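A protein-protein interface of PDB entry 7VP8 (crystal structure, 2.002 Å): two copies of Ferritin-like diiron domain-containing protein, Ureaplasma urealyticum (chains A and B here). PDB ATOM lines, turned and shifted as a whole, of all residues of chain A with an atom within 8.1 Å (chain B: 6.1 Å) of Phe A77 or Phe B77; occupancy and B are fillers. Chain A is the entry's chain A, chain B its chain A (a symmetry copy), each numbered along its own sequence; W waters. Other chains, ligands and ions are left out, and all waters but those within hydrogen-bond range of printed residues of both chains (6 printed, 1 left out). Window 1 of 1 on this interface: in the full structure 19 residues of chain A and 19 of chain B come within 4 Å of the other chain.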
ATOM      1  N   ASN A  14      -4.335 -17.738   8.441  1.00  0.00           N
ATOM      2  CA  ASN A  14      -3.522 -18.835   7.932  1.00  0.00           C
ATOM      3  C   ASN A  14      -2.234 -18.977   8.729  1.00  0.00           C
ATOM      4  O   ASN A  14      -1.832 -20.088   9.093  1.00  0.00           O
ATOM      5  CB  ASN A  14      -3.215 -18.601   6.455  1.00  0.00           C
ATOM      6  CG  ASN A  14      -4.276 -19.179   5.554  1.00  0.00           C
ATOM      7  OD1 ASN A  14      -4.100 -20.259   4.980  1.00  0.00           O
ATOM      8  ND2 ASN A  14      -5.401 -18.481   5.444  1.00  0.00           N
ATOM      9  N   ALA A  15      -1.561 -17.852   8.988  1.00  0.00           N
ATOM     10  CA  ALA A  15      -0.341 -17.884   9.786  1.00  0.00           C
ATOM     11  C   ALA A  15      -0.611 -18.448  11.174  1.00  0.00           C
ATOM     12  O   ALA A  15       0.166 -19.265  11.685  1.00  0.00           O
ATOM     13  CB  ALA A  15       0.263 -16.475   9.883  1.00  0.00           C
ATOM     14  N   TYR A  17      -3.087 -20.452  12.211  1.00  0.00           N
ATOM     15  CA  TYR A  17      -3.371 -21.885  12.121  1.00  0.00           C
ATOM     16  C   TYR A  17      -2.078 -22.685  12.073  1.00  0.00           C
ATOM     17  O   TYR A  17      -1.878 -23.632  12.844  1.00  0.00           O
ATOM     18  CB  TYR A  17      -4.216 -22.175  10.876  1.00  0.00           C
ATOM     19  CG  TYR A  17      -4.522 -23.651  10.673  1.00  0.00           C
ATOM     20  CD1 TYR A  17      -5.518 -24.280  11.412  1.00  0.00           C
ATOM     21  CD2 TYR A  17      -3.803 -24.416   9.749  1.00  0.00           C
ATOM     22  CE1 TYR A  17      -5.804 -25.631  11.235  1.00  0.00           C
ATOM     23  CE2 TYR A  17      -4.079 -25.775   9.570  1.00  0.00           C
ATOM     24  CZ  TYR A  17      -5.086 -26.370  10.316  1.00  0.00           C
ATOM     25  OH  TYR A  17      -5.372 -27.712  10.158  1.00  0.00           O
ATOM     26  N   ASN A  18      -1.183 -22.308  11.163  1.00  0.00           N
ATOM     27  CA  ASN A  18       0.077 -23.017  11.018  1.00  0.00           C
ATOM     28  C   ASN A  18       0.958 -22.859  12.253  1.00  0.00           C
ATOM     29  O   ASN A  18       1.663 -23.803  12.628  1.00  0.00           O
ATOM     30  CB  ASN A  18       0.786 -22.530   9.749  1.00  0.00           C
ATOM     31  CG  ASN A  18       0.202 -23.174   8.487  1.00  0.00           C
ATOM     32  OD1 ASN A  18       0.428 -24.352   8.227  1.00  0.00           O
ATOM     33  ND2 ASN A  18      -0.583 -22.413   7.727  1.00  0.00           N
ATOM     34  N   LEU A  19       0.907 -21.700  12.919  1.00  0.00           N
ATOM     35  CA  LEU A  19       1.729 -21.513  14.112  1.00  0.00           C
ATOM     36  C   LEU A  19       1.332 -22.497  15.203  1.00  0.00           C
ATOM     37  O   LEU A  19       2.187 -23.014  15.931  1.00  0.00           O
ATOM     38  CB  LEU A  19       1.613 -20.074  14.622  1.00  0.00           C
ATOM     39  CG  LEU A  19       2.486 -19.760  15.854  1.00  0.00           C
ATOM     40  CD1 LEU A  19       3.950 -20.029  15.556  1.00  0.00           C
ATOM     41  CD2 LEU A  19       2.305 -18.331  16.319  1.00  0.00           C
ATOM     42  N   ASN A  20       0.036 -22.774  15.333  1.00  0.00           N
ATOM     43  CA  ASN A  20      -0.406 -23.686  16.384  1.00  0.00           C
ATOM     44  C   ASN A  20       0.004 -25.122  16.086  1.00  0.00           C
ATOM     45  O   ASN A  20       0.405 -25.858  16.997  1.00  0.00           O
ATOM     46  CB  ASN A  20      -1.915 -23.558  16.582  1.00  0.00           C
ATOM     47  CG  ASN A  20      -2.262 -22.393  17.500  1.00  0.00           C
ATOM     48  OD1 ASN A  20      -2.047 -22.467  18.708  1.00  0.00           O
ATOM     49  ND2 ASN A  20      -2.753 -21.296  16.925  1.00  0.00           N
ATOM     50  N   LEU A  21      -0.075 -25.540  14.820  1.00  0.00           N
ATOM     51  CA  LEU A  21       0.455 -26.852  14.452  1.00  0.00           C
ATOM     52  C   LEU A  21       1.957 -26.926  14.702  1.00  0.00           C
ATOM     53  O   LEU A  21       2.458 -27.911  15.257  1.00  0.00           O
ATOM     54  CB  LEU A  21       0.142 -27.155  12.987  1.00  0.00           C
ATOM     55  CG  LEU A  21      -1.292 -27.558  12.650  1.00  0.00           C
ATOM     56  CD1 LEU A  21      -1.487 -27.591  11.139  1.00  0.00           C
ATOM     57  CD2 LEU A  21      -1.593 -28.917  13.265  1.00  0.00           C
ATOM     58  N   GLU A  22       2.687 -25.886  14.307  1.00  0.00           N
ATOM     59  CA  GLU A  22       4.129 -25.860  14.518  1.00  0.00           C
ATOM     60  C   GLU A  22       4.476 -25.900  16.000  1.00  0.00           C
ATOM     61  O   GLU A  22       5.254 -26.752  16.441  1.00  0.00           O
ATOM     62  CB  GLU A  22       4.723 -24.617  13.867  1.00  0.00           C
ATOM     63  CG  GLU A  22       6.226 -24.512  14.013  1.00  0.00           C
ATOM     64  CD  GLU A  22       6.750 -23.178  13.505  1.00  0.00           C
ATOM     65  OE1 GLU A  22       6.025 -22.503  12.740  1.00  0.00           O
ATOM     66  OE2 GLU A  22       7.877 -22.803  13.872  1.00  0.00           O
ATOM     67  N   LEU A  23       3.918 -24.966  16.783  1.00  0.00           N
ATOM     68  CA  LEU A  23       4.233 -24.903  18.209  1.00  0.00           C
ATOM     69  C   LEU A  23       3.720 -26.123  18.960  1.00  0.00           C
ATOM     70  O   LEU A  23       4.357 -26.562  19.921  1.00  0.00           O
ATOM     71  CB  LEU A  23       3.645 -23.632  18.838  1.00  0.00           C
ATOM     72  CG  LEU A  23       4.312 -22.312  18.461  1.00  0.00           C
ATOM     73  CD1 LEU A  23       3.815 -21.181  19.371  1.00  0.00           C
ATOM     74  CD2 LEU A  23       5.820 -22.445  18.542  1.00  0.00           C
ATOM     75  N   GLY A  24       2.573 -26.673  18.562  1.00  0.00           N
ATOM     76  CA  GLY A  24       2.108 -27.888  19.210  1.00  0.00           C
ATOM     77  C   GLY A  24       3.112 -29.019  19.084  1.00  0.00           C
ATOM     78  O   GLY A  24       3.354 -29.759  20.040  1.00  0.00           O
ATOM     79  N   SER A  25       3.709 -29.160  17.894  1.00  0.00           N
ATOM     80  CA  SER A  25       4.730 -30.176  17.647  1.00  0.00           C
ATOM     81  C   SER A  25       6.011 -29.869  18.406  1.00  0.00           C
ATOM     82  O   SER A  25       6.653 -30.780  18.948  1.00  0.00           O
ATOM     83  CB  SER A  25       5.023 -30.258  16.143  1.00  0.00           C
ATOM     84  OG  SER A  25       3.842 -30.540  15.397  1.00  0.00           O
ATOM     85  N   VAL A  26       6.408 -28.592  18.436  1.00  0.00           N
ATOM     86  CA  VAL A  26       7.597 -28.190  19.191  1.00  0.00           C
ATOM     87  C   VAL A  26       7.407 -28.486  20.674  1.00  0.00           C
ATOM     88  O   VAL A  26       8.284 -29.067  21.333  1.00  0.00           O
ATOM     89  CB  VAL A  26       7.904 -26.699  18.949  1.00  0.00           C
ATOM     90  CG1 VAL A  26       8.969 -26.208  19.922  1.00  0.00           C
ATOM     91  CG2 VAL A  26       8.344 -26.461  17.496  1.00  0.00           C
ATOM     92  N   LEU A  55      -2.266 -28.214  19.218  1.00  0.00           N
ATOM     93  CA  LEU A  55      -2.501 -29.210  18.173  1.00  0.00           C
ATOM     94  C   LEU A  55      -3.969 -29.564  18.021  1.00  0.00           C
ATOM     95  O   LEU A  55      -4.344 -30.172  17.009  1.00  0.00           O
ATOM     96  CB  LEU A  55      -1.739 -30.504  18.478  1.00  0.00           C
ATOM     97  CG  LEU A  55      -0.229 -30.532  18.318  1.00  0.00           C
ATOM     98  CD1 LEU A  55       0.290 -31.893  18.722  1.00  0.00           C
ATOM     99  CD2 LEU A  55       0.157 -30.221  16.873  1.00  0.00           C
ATOM    100  N   HIS A  74      -4.499 -23.034   4.050  1.00  0.00           N
ATOM    101  CA  HIS A  74      -3.493 -23.954   3.541  1.00  0.00           C
ATOM    102  C   HIS A  74      -2.485 -24.264   4.633  1.00  0.00           C
ATOM    103  O   HIS A  74      -2.122 -23.391   5.421  1.00  0.00           O
ATOM    104  CB  HIS A  74      -2.817 -23.374   2.299  1.00  0.00           C
ATOM    105  CG  HIS A  74      -3.734 -23.329   1.115  1.00  0.00           C
ATOM    106  ND1 HIS A  74      -4.402 -22.184   0.734  1.00  0.00           N
ATOM    107  CD2 HIS A  74      -4.145 -24.305   0.268  1.00  0.00           C
ATOM    108  CE1 HIS A  74      -5.165 -22.450  -0.312  1.00  0.00           C
ATOM    109  NE2 HIS A  74      -5.027 -23.729  -0.615  1.00  0.00           N
ATOM    110  N   THR A  75      -2.053 -25.518   4.684  1.00  0.00           N
ATOM    111  CA  THR A  75      -1.125 -25.990   5.704  1.00  0.00           C
ATOM    112  C   THR A  75       0.278 -26.046   5.120  1.00  0.00           C
ATOM    113  O   THR A  75       0.529 -26.796   4.163  1.00  0.00           O
ATOM    114  CB  THR A  75      -1.525 -27.374   6.224  1.00  0.00           C
ATOM    115  OG1 THR A  75      -2.818 -27.303   6.839  1.00  0.00           O
ATOM    116  CG2 THR A  75      -0.502 -27.864   7.251  1.00  0.00           C
ATOM    117  N   LYS A  76       1.193 -25.280   5.711  1.00  0.00           N
ATOM    118  CA  LYS A  76       2.605 -25.381   5.351  1.00  0.00           C
ATOM    119  C   LYS A  76       3.426 -24.862   6.517  1.00  0.00           C
ATOM    120  O   LYS A  76       3.292 -23.695   6.899  1.00  0.00           O
ATOM    121  CB  LYS A  76       2.918 -24.603   4.071  1.00  0.00           C
ATOM    122  CG  LYS A  76       4.404 -24.615   3.710  1.00  0.00           C
ATOM    123  CD  LYS A  76       4.679 -23.844   2.440  1.00  0.00           C
ATOM    124  CE  LYS A  76       6.161 -23.822   2.128  1.00  0.00           C
ATOM    125  NZ  LYS A  76       6.908 -22.972   3.114  1.00  0.00           N
ATOM    126  N   PHE A  77       4.245 -25.729   7.101  1.00  0.00           N
ATOM    127  CA  PHE A  77       5.132 -25.338   8.185  1.00  0.00           C
ATOM    128  C   PHE A  77       6.206 -26.407   8.300  1.00  0.00           C
ATOM    129  O   PHE A  77       6.081 -27.508   7.755  1.00  0.00           O
ATOM    130  CB  PHE A  77       4.376 -25.175   9.514  1.00  0.00           C
ATOM    131  CG  PHE A  77       3.842 -26.472  10.065  1.00  0.00           C
ATOM    132  CD1 PHE A  77       2.637 -26.992   9.595  1.00  0.00           C
ATOM    133  CD2 PHE A  77       4.540 -27.175  11.036  1.00  0.00           C
ATOM    134  CE1 PHE A  77       2.131 -28.200  10.090  1.00  0.00           C
ATOM    135  CE2 PHE A  77       4.041 -28.393  11.541  1.00  0.00           C
ATOM    136  CZ  PHE A  77       2.832 -28.901  11.063  1.00  0.00           C
ATOM    137  N   SER A  78       7.263 -26.077   9.032  1.00  0.00           N
ATOM    138  CA  SER A  78       8.318 -27.039   9.294  1.00  0.00           C
ATOM    139  C   SER A  78       8.763 -26.906  10.741  1.00  0.00           C
ATOM    140  O   SER A  78       8.716 -25.818  11.326  1.00  0.00           O
ATOM    141  CB  SER A  78       9.510 -26.845   8.341  1.00  0.00           C
ATOM    142  OG  SER A  78       9.982 -25.523   8.448  1.00  0.00           O
ATOM    143  N   VAL A  79       9.192 -28.037  11.303  1.00  0.00           N
ATOM    144  CA  VAL A  79       9.616 -28.162  12.692  1.00  0.00           C
ATOM    145  C   VAL A  79      10.986 -28.828  12.697  1.00  0.00           C
ATOM    146  O   VAL A  79      11.194 -29.824  11.997  1.00  0.00           O
ATOM    147  CB  VAL A  79       8.618 -29.001  13.519  1.00  0.00           C
ATOM    148  CG1 VAL A  79       9.140 -29.228  14.934  1.00  0.00           C
ATOM    149  CG2 VAL A  79       7.241 -28.337  13.543  1.00  0.00           C
ATOM    150  N   ASP A  80      11.913 -28.275  13.480  1.00  0.00           N
ATOM    151  CA  ASP A  80      13.241 -28.863  13.690  1.00  0.00           C
ATOM    152  C   ASP A  80      13.687 -28.396  15.079  1.00  0.00           C
ATOM    153  O   ASP A  80      14.272 -27.321  15.224  1.00  0.00           O
ATOM    154  CB  ASP A  80      14.218 -28.440  12.601  1.00  0.00           C
ATOM    155  CG  ASP A  80      15.595 -29.083  12.755  1.00  0.00           C
ATOM    156  OD1 ASP A  80      15.832 -29.823  13.739  1.00  0.00           O
ATOM    157  OD2 ASP A  80      16.441 -28.859  11.865  1.00  0.00           O
ATOM    158  N   VAL A  81      13.369 -29.192  16.096  1.00  0.00           N
ATOM    159  CA  VAL A  81      13.538 -28.732  17.472  1.00  0.00           C
ATOM    160  C   VAL A  81      15.003 -28.904  17.855  1.00  0.00           C
ATOM    161  O   VAL A  81      15.486 -30.023  18.043  1.00  0.00           O
ATOM    162  CB  VAL A  81      12.611 -29.468  18.443  1.00  0.00           C
ATOM    163  CG1 VAL A  81      12.843 -28.950  19.859  1.00  0.00           C
ATOM    164  CG2 VAL A  81      11.149 -29.251  18.029  1.00  0.00           C
ATOM    165  N   ASN B  18       8.068 -39.030  13.910  1.00  0.00           N
ATOM    166  CA  ASN B  18       7.920 -37.871  13.045  1.00  0.00           C
ATOM    167  C   ASN B  18       6.863 -38.101  11.970  1.00  0.00           C
ATOM    168  O   ASN B  18       6.142 -37.163  11.610  1.00  0.00           O
ATOM    169  CB  ASN B  18       9.282 -37.520  12.436  1.00  0.00           C
ATOM    170  CG  ASN B  18      10.170 -36.754  13.424  1.00  0.00           C
ATOM    171  OD1 ASN B  18       9.928 -35.582  13.697  1.00  0.00           O
ATOM    172  ND2 ASN B  18      11.168 -37.429  13.991  1.00  0.00           N
ATOM    173  N   LEU B  19       6.727 -39.335  11.474  1.00  0.00           N
ATOM    174  CA  LEU B  19       5.719 -39.597  10.449  1.00  0.00           C
ATOM    175  C   LEU B  19       4.319 -39.339  10.988  1.00  0.00           C
ATOM    176  O   LEU B  19       3.449 -38.828  10.273  1.00  0.00           O
ATOM    177  CB  LEU B  19       5.839 -41.035   9.937  1.00  0.00           C
ATOM    178  CG  LEU B  19       4.847 -41.397   8.811  1.00  0.00           C
ATOM    179  CD1 LEU B  19       5.021 -40.466   7.625  1.00  0.00           C
ATOM    180  CD2 LEU B  19       5.003 -42.836   8.369  1.00  0.00           C
ATOM    181  N   LEU B  21       3.420 -37.229  13.463  1.00  0.00           N
ATOM    182  CA  LEU B  21       3.225 -35.782  13.526  1.00  0.00           C
ATOM    183  C   LEU B  21       2.978 -35.200  12.138  1.00  0.00           C
ATOM    184  O   LEU B  21       2.074 -34.378  11.949  1.00  0.00           O
ATOM    185  CB  LEU B  21       4.438 -35.115  14.175  1.00  0.00           C
ATOM    186  CG  LEU B  21       4.571 -35.238  15.692  1.00  0.00           C
ATOM    187  CD1 LEU B  21       5.936 -34.732  16.142  1.00  0.00           C
ATOM    188  CD2 LEU B  21       3.454 -34.452  16.363  1.00  0.00           C
ATOM    189  N   GLU B  22       3.767 -35.626  11.156  1.00  0.00           N
ATOM    190  CA  GLU B  22       3.596 -35.138   9.793  1.00  0.00           C
ATOM    191  C   GLU B  22       2.228 -35.511   9.237  1.00  0.00           C
ATOM    192  O   GLU B  22       1.484 -34.646   8.764  1.00  0.00           O
ATOM    193  CB  GLU B  22       4.700 -35.695   8.903  1.00  0.00           C
ATOM    194  CG  GLU B  22       4.621 -35.225   7.467  1.00  0.00           C
ATOM    195  CD  GLU B  22       5.632 -35.937   6.583  1.00  0.00           C
ATOM    196  OE1 GLU B  22       6.600 -36.515   7.127  1.00  0.00           O
ATOM    197  OE2 GLU B  22       5.457 -35.928   5.352  1.00  0.00           O
ATOM    198  N   SER B  25      -0.835 -33.799  10.815  1.00  0.00           N
ATOM    199  CA  SER B  25      -1.016 -32.444  10.300  1.00  0.00           C
ATOM    200  C   SER B  25      -1.574 -32.459   8.887  1.00  0.00           C
ATOM    201  O   SER B  25      -2.436 -31.637   8.543  1.00  0.00           O
ATOM    202  CB  SER B  25       0.327 -31.700  10.321  1.00  0.00           C
ATOM    203  OG  SER B  25       0.885 -31.670  11.632  1.00  0.00           O
ATOM    204  N   THR B  75      12.672 -34.310  17.002  1.00  0.00           N
ATOM    205  CA  THR B  75      11.555 -33.914  16.154  1.00  0.00           C
ATOM    206  C   THR B  75      12.075 -33.081  14.993  1.00  0.00           C
ATOM    207  O   THR B  75      12.646 -31.999  15.205  1.00  0.00           O
ATOM    208  CB  THR B  75      10.514 -33.114  16.941  1.00  0.00           C
ATOM    209  OG1 THR B  75       9.971 -33.926  17.990  1.00  0.00           O
ATOM    210  CG2 THR B  75       9.383 -32.666  16.011  1.00  0.00           C
ATOM    211  N   LYS B  76      11.854 -33.567  13.773  1.00  0.00           N
ATOM    212  CA  LYS B  76      12.152 -32.774  12.583  1.00  0.00           C
ATOM    213  C   LYS B  76      11.305 -33.304  11.441  1.00  0.00           C
ATOM    214  O   LYS B  76      11.429 -34.474  11.067  1.00  0.00           O
ATOM    215  CB  LYS B  76      13.640 -32.824  12.229  1.00  0.00           C
ATOM    216  CG  LYS B  76      13.975 -32.076  10.939  1.00  0.00           C
ATOM    217  CD  LYS B  76      15.452 -32.139  10.621  1.00  0.00           C
ATOM    218  CE  LYS B  76      15.756 -31.438   9.313  1.00  0.00           C
ATOM    219  NZ  LYS B  76      15.207 -32.208   8.148  1.00  0.00           N
ATOM    220  N   PHE B  77      10.423 -32.462  10.913  1.00  0.00           N
ATOM    221  CA  PHE B  77       9.599 -32.827   9.772  1.00  0.00           C
ATOM    222  C   PHE B  77       9.067 -31.540   9.166  1.00  0.00           C
ATOM    223  O   PHE B  77       9.115 -30.470   9.780  1.00  0.00           O
ATOM    224  CB  PHE B  77       8.446 -33.763  10.174  1.00  0.00           C
ATOM    225  CG  PHE B  77       7.411 -33.100  11.046  1.00  0.00           C
ATOM    226  CD1 PHE B  77       7.620 -32.983  12.419  1.00  0.00           C
ATOM    227  CD2 PHE B  77       6.243 -32.587  10.502  1.00  0.00           C
ATOM    228  CE1 PHE B  77       6.673 -32.362  13.243  1.00  0.00           C
ATOM    229  CE2 PHE B  77       5.282 -31.960  11.320  1.00  0.00           C
ATOM    230  CZ  PHE B  77       5.503 -31.850  12.694  1.00  0.00           C
ATOM    231  N   SER B  78       8.540 -31.655   7.954  1.00  0.00           N
ATOM    232  CA  SER B  78       7.917 -30.519   7.300  1.00  0.00           C
ATOM    233  C   SER B  78       6.652 -30.983   6.595  1.00  0.00           C
ATOM    234  O   SER B  78       6.561 -32.127   6.136  1.00  0.00           O
ATOM    235  CB  SER B  78       8.875 -29.844   6.304  1.00  0.00           C
ATOM    236  OG  SER B  78       9.319 -30.796   5.365  1.00  0.00           O
ATOM    237  N   VAL B  79       5.682 -30.071   6.525  1.00  0.00           N
ATOM    238  CA  VAL B  79       4.366 -30.306   5.945  1.00  0.00           C
ATOM    239  C   VAL B  79       4.099 -29.195   4.939  1.00  0.00           C
ATOM    240  O   VAL B  79       4.335 -28.020   5.237  1.00  0.00           O
ATOM    241  CB  VAL B  79       3.261 -30.318   7.025  1.00  0.00           C
ATOM    242  CG1 VAL B  79       1.880 -30.438   6.388  1.00  0.00           C
ATOM    243  CG2 VAL B  79       3.499 -31.442   8.033  1.00  0.00           C
ATOM    244  N   ASP B  80       3.615 -29.568   3.754  1.00  0.00           N
ATOM    245  CA  ASP B  80       3.194 -28.614   2.721  1.00  0.00           C
ATOM    246  C   ASP B  80       2.119 -29.336   1.903  1.00  0.00           C
ATOM    247  O   ASP B  80       2.428 -30.048   0.947  1.00  0.00           O
ATOM    248  CB  ASP B  80       4.368 -28.167   1.860  1.00  0.00           C
ATOM    249  CG  ASP B  80       3.976 -27.126   0.814  1.00  0.00           C
ATOM    250  OD1 ASP B  80       2.777 -26.775   0.701  1.00  0.00           O
ATOM    251  OD2 ASP B  80       4.885 -26.640   0.111  1.00  0.00           O
HETATM  252  O   HOH W   1       0.469 -25.621   1.359  1.00  0.00           O
HETATM  253  O   HOH W   2       7.505 -33.523  18.996  1.00  0.00           O
HETATM  254  O   HOH W   3       6.864 -26.962   4.799  1.00  0.00           O
HETATM  255  O   HOH W   4      14.274 -32.499  18.743  1.00  0.00           O
HETATM  256  O   HOH W   5      12.043 -29.516   9.372  1.00  0.00           O
HETATM  257  O   HOH W   6      -3.591 -29.016   8.769  1.00  0.00           O
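N of Val A81 is in hydrogen-bond range of O of Thr B75, 3.0 Å away. The backbone carbonyl oxygen (O) of Phe A77 sits at hydrogen-bond distance from the backbone NH (N) of Val B79, 2.9 Å away. The backbone carbonyl oxygen (O) of Phe B77 sits at hydrogen-bond distance from the backbone NH (N) of Val A79 (2.9 Å).
The backbone carbonyl oxygen (O) of Leu A21 sits at hydrogen-bond distance from the side-chain hydroxyl (OG) of Ser A25. O of Leu B21 sits at hydrogen-bond distance from OG of Ser B25 (3.0 Å). The side-chain amide oxygen (OD1) of Asn B18 sits at hydrogen-bond distance from the backbone NH (N) of Lys B76 (2.8 Å). The side-chain amide oxygen of Asn A18 sits at hydrogen-bond distance from the backbone NH of Lys A76, at 2.8 Å.
Among the printed residues, pairs that only touch across the chains: Val A79 with Lys B76 (3.2 Å), Lys A76 with Val B79 (3.2 Å), Ser A25 with Phe B77 (3.4 Å), Phe A77 with Ser B25 (3.4 Å), Asp A80 with Thr B75 (3.5 Å), Thr A75 with Asp B80 (3.5 Å), Ser A78 with Phe B77 (3.6 Å), Phe A77 with Ser B78 (3.6 Å), Val A79 with Thr B75 (3.6 Å), Thr A75 with Val B79 (3.6 Å), Asp A80 with Lys B76 (3.6 Å), Lys A76 with Asp B80 (3.6 Å), Ser A78 with Ser B78 (3.7 Å) and Phe A77 with Phe B77 (3.8 Å).
Of the printed residues of chain B, Phe A77 touches Ser B25, Phe B77, Ser B78 and Val B79. Phe B77 touches just these residues of chain A: Ser A25, Phe A77, Ser A78 and Val A79. Of chain A, only Phe A77 and Ser A78 come within 4 Å of Ser B78. Of the printed residues of chain A, Thr B75 touches Val A79, Asp A80 and Val A81. Of the printed residues of chain B, Thr A75 touches Val B79 (3.6 Å) and Asp B80 (3.5 Å). Printed residues of chain B within 4 Å of Lys A76: Val B79 (3.2 Å) and Asp B80 (3.6 Å). Of the printed residues of chain A, Asp B80 touches Thr A75 and Lys A76. Printed residues of chain B within 4 Å of Ser A25: Phe B77 (3.4 Å). Leu A55 touches none of the printed residues of chain B. Asn A14 touches none of the printed residues of chain B. The nearest residue of chain A that does not touch Phe B77 is Asp A80 (5.1 Å). The nearest printed residue of chain B that does not touch Lys A76 is Ser B78 (6.9 Å).
Printed residues of chain A that touch a printed residue of chain B: Ser A25, Thr A75, Lys A76, Phe A77, Ser A78, Val A79, Asp A80 and Val A81. Hydrophobic or aromatic side chains of chain B within 4 Å of the printed part of chain A: Phe B77 and Val B79. Among the printed residues, 17 pairs touch across the chains. Among the printed residues, no Asp or Glu carboxylate lies within 4 Å of a Lys or Arg side-chain nitrogen of the other chain.
Lys A76 touches Val B79, and with the chains exchanged Val A79 touches Lys B76. Lys A76 touches Asp B80, and with the chains exchanged Asp A80 touches Lys B76. Phe A77 touches Ser B78, and with the chains exchanged Ser A78 touches Phe B77. Phe A77 touches Val B79, and with the chains exchanged Val A79 touches Phe B77. Positions printed for both chains: 18, 19, 21, 22, 25, 75, 76, 77, 78, 79 and 80. Of the 17 pairs that touch across the chains among the printed residues, 16 have their exchanged pair printed and touching as well.
Water W6 lies within hydrogen-bond range of OH of Tyr A17, OG1 of Thr A75 and O of Ser B25. Water W1 lies within hydrogen-bond range of the side-chain carboxylate of Asp B80 and the backbone carbonyl oxygen of Thr A75. Water W2 lies within hydrogen-bond range of the side-chain hydroxyl of Thr B75 (2.7 Å) and the backbone carbonyl oxygen of Ser A25 (2.9 Å). Water W5 bridges O of Val A79 and O of Phe B77. Water W3 lies within hydrogen-bond range of the backbone carbonyl oxygen (O) of Val B79 and the backbone carbonyl oxygen (O) of Phe A77. Water W4 bridges O of Val A81 (2.8 Å) and N of Thr B75 (3.0 Å).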
